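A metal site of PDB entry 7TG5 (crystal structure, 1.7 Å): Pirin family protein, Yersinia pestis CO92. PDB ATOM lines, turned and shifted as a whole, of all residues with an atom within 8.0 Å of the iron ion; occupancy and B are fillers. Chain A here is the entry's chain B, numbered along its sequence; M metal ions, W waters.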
ATOM      1  N   VAL A  19      -0.615  16.680 -14.571  1.00  0.00           N
ATOM      2  CA  VAL A  19      -1.495  16.338 -15.686  1.00  0.00           C
ATOM      3  C   VAL A  19      -2.081  14.971 -15.368  1.00  0.00           C
ATOM      4  O   VAL A  19      -1.384  13.947 -15.418  1.00  0.00           O
ATOM      5  CB  VAL A  19      -0.732  16.339 -17.016  1.00  0.00           C
ATOM      6  CG1 VAL A  19      -1.612  15.805 -18.112  1.00  0.00           C
ATOM      7  CG2 VAL A  19      -0.259  17.745 -17.345  1.00  0.00           C
ATOM      8  N   VAL A  61      -4.000   9.948 -17.573  1.00  0.00           N
ATOM      9  CA  VAL A  61      -4.904  10.963 -18.085  1.00  0.00           C
ATOM     10  C   VAL A  61      -6.053  10.270 -18.806  1.00  0.00           C
ATOM     11  O   VAL A  61      -5.842   9.318 -19.562  1.00  0.00           O
ATOM     12  CB  VAL A  61      -4.187  11.967 -19.006  1.00  0.00           C
ATOM     13  CG1 VAL A  61      -3.082  12.643 -18.264  1.00  0.00           C
ATOM     14  CG2 VAL A  61      -3.633  11.282 -20.247  1.00  0.00           C
ATOM     15  N   GLY A  62      -7.263  10.749 -18.577  1.00  0.00           N
ATOM     16  CA  GLY A  62      -8.418  10.198 -19.245  1.00  0.00           C
ATOM     17  C   GLY A  62      -8.378  10.433 -20.743  1.00  0.00           C
ATOM     18  O   GLY A  62      -7.545  11.164 -21.269  1.00  0.00           O
ATOM     19  N   GLN A  63      -9.289   9.763 -21.435  1.00  0.00           N
ATOM     20  CA  GLN A  63      -9.385   9.901 -22.878  1.00  0.00           C
ATOM     21  C   GLN A  63      -9.631  11.355 -23.242  1.00  0.00           C
ATOM     22  O   GLN A  63     -10.344  12.085 -22.549  1.00  0.00           O
ATOM     23  CB  GLN A  63     -10.512   9.026 -23.432  1.00  0.00           C
ATOM     24  CG  GLN A  63     -10.533   8.937 -24.946  1.00  0.00           C
ATOM     25  CD  GLN A  63     -11.697   8.128 -25.465  1.00  0.00           C
ATOM     26  OE1 GLN A  63     -12.854   8.506 -25.280  1.00  0.00           O
ATOM     27  NE2 GLN A  63     -11.398   7.016 -26.114  1.00  0.00           N
ATOM     28  N   HIS A  64      -9.020  11.797 -24.338  1.00  0.00           N
ATOM     29  CA  HIS A  64      -9.131  13.176 -24.787  1.00  0.00           C
ATOM     30  C   HIS A  64      -8.800  13.214 -26.267  1.00  0.00           C
ATOM     31  O   HIS A  64      -8.104  12.331 -26.780  1.00  0.00           O
ATOM     32  CB  HIS A  64      -8.203  14.098 -23.995  1.00  0.00           C
ATOM     33  CG  HIS A  64      -6.765  13.710 -24.058  1.00  0.00           C
ATOM     34  ND1 HIS A  64      -6.241  12.671 -23.317  1.00  0.00           N
ATOM     35  CD2 HIS A  64      -5.736  14.206 -24.780  1.00  0.00           C
ATOM     36  CE1 HIS A  64      -4.952  12.549 -23.576  1.00  0.00           C
ATOM     37  NE2 HIS A  64      -4.620  13.478 -24.461  1.00  0.00           N
ATOM     38  N   PRO A  65      -9.303  14.216 -26.990  1.00  0.00           N
ATOM     39  CA  PRO A  65      -9.058  14.293 -28.427  1.00  0.00           C
ATOM     40  C   PRO A  65      -7.742  14.980 -28.768  1.00  0.00           C
ATOM     41  O   PRO A  65      -7.167  15.730 -27.975  1.00  0.00           O
ATOM     42  CB  PRO A  65     -10.249  15.128 -28.920  1.00  0.00           C
ATOM     43  CG  PRO A  65     -10.530  16.030 -27.789  1.00  0.00           C
ATOM     44  CD  PRO A  65     -10.272  15.231 -26.541  1.00  0.00           C
ATOM     45  N   HIS A  66      -7.278  14.698 -29.985  1.00  0.00           N
ATOM     46  CA  HIS A  66      -6.127  15.378 -30.573  1.00  0.00           C
ATOM     47  C   HIS A  66      -6.377  15.470 -32.072  1.00  0.00           C
ATOM     48  O   HIS A  66      -6.868  14.523 -32.680  1.00  0.00           O
ATOM     49  CB  HIS A  66      -4.820  14.625 -30.305  1.00  0.00           C
ATOM     50  CG  HIS A  66      -4.231  14.870 -28.961  1.00  0.00           C
ATOM     51  ND1 HIS A  66      -4.569  15.959 -28.185  1.00  0.00           N
ATOM     52  CD2 HIS A  66      -3.319  14.172 -28.247  1.00  0.00           C
ATOM     53  CE1 HIS A  66      -3.890  15.918 -27.050  1.00  0.00           C
ATOM     54  NE2 HIS A  66      -3.123  14.839 -27.068  1.00  0.00           N
ATOM     55  N   PHE A  69      -1.626  17.380 -35.392  1.00  0.00           N
ATOM     56  CA  PHE A  69      -0.205  17.367 -35.070  1.00  0.00           C
ATOM     57  C   PHE A  69       0.192  15.963 -34.628  1.00  0.00           C
ATOM     58  O   PHE A  69      -0.593  15.018 -34.741  1.00  0.00           O
ATOM     59  CB  PHE A  69       0.101  18.433 -34.011  1.00  0.00           C
ATOM     60  CG  PHE A  69      -0.707  18.297 -32.754  1.00  0.00           C
ATOM     61  CD1 PHE A  69      -1.941  18.928 -32.627  1.00  0.00           C
ATOM     62  CD2 PHE A  69      -0.261  17.535 -31.692  1.00  0.00           C
ATOM     63  CE1 PHE A  69      -2.689  18.803 -31.479  1.00  0.00           C
ATOM     64  CE2 PHE A  69      -1.008  17.398 -30.537  1.00  0.00           C
ATOM     65  CZ  PHE A  69      -2.224  18.038 -30.441  1.00  0.00           C
ATOM     66  N   THR A  71       2.336  13.611 -31.469  1.00  0.00           N
ATOM     67  CA  THR A  71       2.740  13.551 -30.071  1.00  0.00           C
ATOM     68  C   THR A  71       3.836  12.494 -29.917  1.00  0.00           C
ATOM     69  O   THR A  71       3.685  11.375 -30.413  1.00  0.00           O
ATOM     70  CB  THR A  71       1.569  13.231 -29.155  1.00  0.00           C
ATOM     71  OG1 THR A  71       0.532  14.208 -29.347  1.00  0.00           O
ATOM     72  CG2 THR A  71       1.994  13.269 -27.716  1.00  0.00           C
ATOM     73  N   HIS A  82      -0.433   3.103 -23.866  1.00  0.00           N
ATOM     74  CA  HIS A  82      -1.178   4.001 -24.733  1.00  0.00           C
ATOM     75  C   HIS A  82      -2.322   3.238 -25.390  1.00  0.00           C
ATOM     76  O   HIS A  82      -2.207   2.042 -25.676  1.00  0.00           O
ATOM     77  CB  HIS A  82      -0.248   4.618 -25.789  1.00  0.00           C
ATOM     78  CG  HIS A  82      -0.961   5.275 -26.934  1.00  0.00           C
ATOM     79  ND1 HIS A  82      -1.156   4.641 -28.141  1.00  0.00           N
ATOM     80  CD2 HIS A  82      -1.507   6.506 -27.062  1.00  0.00           C
ATOM     81  CE1 HIS A  82      -1.805   5.454 -28.958  1.00  0.00           C
ATOM     82  NE2 HIS A  82      -2.026   6.596 -28.327  1.00  0.00           N
ATOM     83  N   MET A 100       3.142   9.270 -32.260  1.00  0.00           N
ATOM     84  CA  MET A 100       1.728   9.154 -32.628  1.00  0.00           C
ATOM     85  C   MET A 100       1.287  10.305 -33.502  1.00  0.00           C
ATOM     86  O   MET A 100       1.426  11.458 -33.119  1.00  0.00           O
ATOM     87  CB  MET A 100       0.860   9.107 -31.376  1.00  0.00           C
ATOM     88  CG  MET A 100      -0.605   8.874 -31.665  1.00  0.00           C
ATOM     89  SD  MET A 100      -1.745   9.303 -30.153  1.00  0.00           S
ATOM     90  CE  MET A 100      -1.400  11.213 -30.036  1.00  0.00           C
ATOM     91  N   ALA A 102      -1.624  12.312 -34.604  1.00  0.00           N
ATOM     92  CA  ALA A 102      -3.032  12.601 -34.347  1.00  0.00           C
ATOM     93  C   ALA A 102      -3.757  12.937 -35.644  1.00  0.00           C
ATOM     94  O   ALA A 102      -4.810  12.363 -35.949  1.00  0.00           O
ATOM     95  CB  ALA A 102      -3.156  13.747 -33.345  1.00  0.00           C
ATOM     96  N   ILE A 106      -7.451  11.753 -33.219  1.00  0.00           N
ATOM     97  CA  ILE A 106      -7.259  10.586 -32.373  1.00  0.00           C
ATOM     98  C   ILE A 106      -7.893  10.852 -31.009  1.00  0.00           C
ATOM     99  O   ILE A 106      -7.826  11.969 -30.486  1.00  0.00           O
ATOM    100  CB  ILE A 106      -5.767  10.229 -32.228  1.00  0.00           C
ATOM    101  CG1 ILE A 106      -5.439   8.964 -33.012  1.00  0.00           C
ATOM    102  CG2 ILE A 106      -5.369  10.058 -30.767  1.00  0.00           C
ATOM    103  CD1 ILE A 106      -3.964   8.616 -33.022  1.00  0.00           C
ATOM    104  N   LEU A 107      -8.554   9.836 -30.455  1.00  0.00           N
ATOM    105  CA  LEU A 107      -8.993   9.826 -29.066  1.00  0.00           C
ATOM    106  C   LEU A 107      -8.098   8.850 -28.337  1.00  0.00           C
ATOM    107  O   LEU A 107      -8.170   7.639 -28.588  1.00  0.00           O
ATOM    108  CB  LEU A 107     -10.459   9.413 -28.950  1.00  0.00           C
ATOM    109  CG  LEU A 107     -11.561  10.235 -29.599  1.00  0.00           C
ATOM    110  CD1 LEU A 107     -12.857   9.461 -29.518  1.00  0.00           C
ATOM    111  CD2 LEU A 107     -11.688  11.573 -28.909  1.00  0.00           C
ATOM    112  N   HIS A 108      -7.269   9.341 -27.428  1.00  0.00           N
ATOM    113  CA  HIS A 108      -6.342   8.435 -26.753  1.00  0.00           C
ATOM    114  C   HIS A 108      -6.298   8.724 -25.262  1.00  0.00           C
ATOM    115  O   HIS A 108      -6.692   9.787 -24.785  1.00  0.00           O
ATOM    116  CB  HIS A 108      -4.939   8.505 -27.357  1.00  0.00           C
ATOM    117  CG  HIS A 108      -4.155   9.720 -26.948  1.00  0.00           C
ATOM    118  ND1 HIS A 108      -2.796   9.670 -26.695  1.00  0.00           N
ATOM    119  CD2 HIS A 108      -4.535  11.003 -26.750  1.00  0.00           C
ATOM    120  CE1 HIS A 108      -2.379  10.872 -26.360  1.00  0.00           C
ATOM    121  NE2 HIS A 108      -3.405  11.699 -26.384  1.00  0.00           N
ATOM    122  N   GLU A 109      -5.822   7.718 -24.528  1.00  0.00           N
ATOM    123  CA  GLU A 109      -5.513   7.844 -23.115  1.00  0.00           C
ATOM    124  C   GLU A 109      -4.125   7.288 -22.871  1.00  0.00           C
ATOM    125  O   GLU A 109      -3.639   6.430 -23.610  1.00  0.00           O
ATOM    126  CB  GLU A 109      -6.538   7.118 -22.238  1.00  0.00           C
ATOM    127  CG  GLU A 109      -6.580   5.613 -22.439  1.00  0.00           C
ATOM    128  CD  GLU A 109      -7.474   4.920 -21.425  1.00  0.00           C
ATOM    129  OE1 GLU A 109      -7.777   5.524 -20.387  1.00  0.00           O
ATOM    130  OE2 GLU A 109      -7.875   3.762 -21.683  1.00  0.00           O
ATOM    131  N   GLU A 110      -3.479   7.795 -21.826  1.00  0.00           N
ATOM    132  CA  GLU A 110      -2.119   7.401 -21.477  1.00  0.00           C
ATOM    133  C   GLU A 110      -2.059   7.197 -19.972  1.00  0.00           C
ATOM    134  O   GLU A 110      -2.467   8.089 -19.215  1.00  0.00           O
ATOM    135  CB  GLU A 110      -1.099   8.461 -21.927  1.00  0.00           C
ATOM    136  CG  GLU A 110      -1.001   8.631 -23.435  1.00  0.00           C
ATOM    137  CD  GLU A 110      -0.616  10.041 -23.844  1.00  0.00           C
ATOM    138  OE1 GLU A 110      -1.075  10.995 -23.187  1.00  0.00           O
ATOM    139  OE2 GLU A 110       0.145  10.198 -24.822  1.00  0.00           O
ATOM    140  N   GLN A 127       7.225  14.430 -23.171  1.00  0.00           N
ATOM    141  CA  GLN A 127       6.205  14.469 -24.205  1.00  0.00           C
ATOM    142  C   GLN A 127       6.403  15.723 -25.052  1.00  0.00           C
ATOM    143  O   GLN A 127       6.573  16.821 -24.509  1.00  0.00           O
ATOM    144  CB  GLN A 127       4.800  14.435 -23.608  1.00  0.00           C
ATOM    145  CG  GLN A 127       3.697  14.326 -24.630  1.00  0.00           C
ATOM    146  CD  GLN A 127       2.765  13.167 -24.344  1.00  0.00           C
ATOM    147  OE1 GLN A 127       3.193  12.071 -24.011  1.00  0.00           O
ATOM    148  NE2 GLN A 127       1.457  13.412 -24.474  1.00  0.00           N
ATOM    149  N   TRP A 129       5.061  17.768 -28.656  1.00  0.00           N
ATOM    150  CA  TRP A 129       4.153  17.903 -29.784  1.00  0.00           C
ATOM    151  C   TRP A 129       4.905  18.446 -30.986  1.00  0.00           C
ATOM    152  O   TRP A 129       5.697  19.386 -30.867  1.00  0.00           O
ATOM    153  CB  TRP A 129       2.986  18.847 -29.457  1.00  0.00           C
ATOM    154  CG  TRP A 129       1.999  18.325 -28.456  1.00  0.00           C
ATOM    155  CD1 TRP A 129       2.119  17.199 -27.698  1.00  0.00           C
ATOM    156  CD2 TRP A 129       0.760  18.933 -28.092  1.00  0.00           C
ATOM    157  NE1 TRP A 129       1.019  17.064 -26.869  1.00  0.00           N
ATOM    158  CE2 TRP A 129       0.168  18.117 -27.103  1.00  0.00           C
ATOM    159  CE3 TRP A 129       0.092  20.088 -28.495  1.00  0.00           C
ATOM    160  CZ2 TRP A 129      -1.056  18.420 -26.515  1.00  0.00           C
ATOM    161  CZ3 TRP A 129      -1.127  20.387 -27.916  1.00  0.00           C
ATOM    162  CH2 TRP A 129      -1.686  19.560 -26.939  1.00  0.00           C
ATOM    163  N   PRO A 265      -6.241  20.916 -26.964  1.00  0.00           N
ATOM    164  CA  PRO A 265      -5.623  19.790 -27.668  1.00  0.00           C
ATOM    165  C   PRO A 265      -5.740  19.838 -29.180  1.00  0.00           C
ATOM    166  O   PRO A 265      -5.402  18.846 -29.827  1.00  0.00           O
ATOM    167  CB  PRO A 265      -6.402  18.601 -27.098  1.00  0.00           C
ATOM    168  CG  PRO A 265      -7.772  19.151 -26.872  1.00  0.00           C
ATOM    169  CD  PRO A 265      -7.595  20.595 -26.484  1.00  0.00           C
HETATM  170 FE    FE M   1      -3.000  13.894 -25.373  1.00  0.00          FE
HETATM  171  O   HOH W   1      -0.738  13.285 -25.847  1.00  0.00           O
HETATM  172  O   HOH W   2      -1.973  14.511 -23.876  1.00  0.00           O
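O of Gly 62 sits at hydrogen-bond distance from ND1 of His 64, at 2.9 Å.
ND1 of His 66 lies close to O of Pro 265, 3.4 Å away.
The backbone NH (N) of His 66 sits at hydrogen-bond distance from the backbone carbonyl oxygen (O) of Ile 106, at 2.8 Å.
The side-chain sulfur of Met 100 is in hydrogen-bond range of a ring nitrogen (ND1) of His 108 (3.6 Å).
Water W1 bridges NE2 of Gln 127 (2.6 Å) and OE2 of Glu 110 (3.4 Å).
The iron ion is bound by a ring nitrogen (NE2) of His 64 (1.9 Å), water W2 (1.9 Å), a ring nitrogen (NE2) of His 66 (1.9 Å), water W1 (2.4 Å) and a ring nitrogen (NE2) of His 108 (2.5 Å).
The iron ion has five donor atoms within binding distance.
The nearest printed residue that does not touch the iron ion is Glu 110 (4.1 Å).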
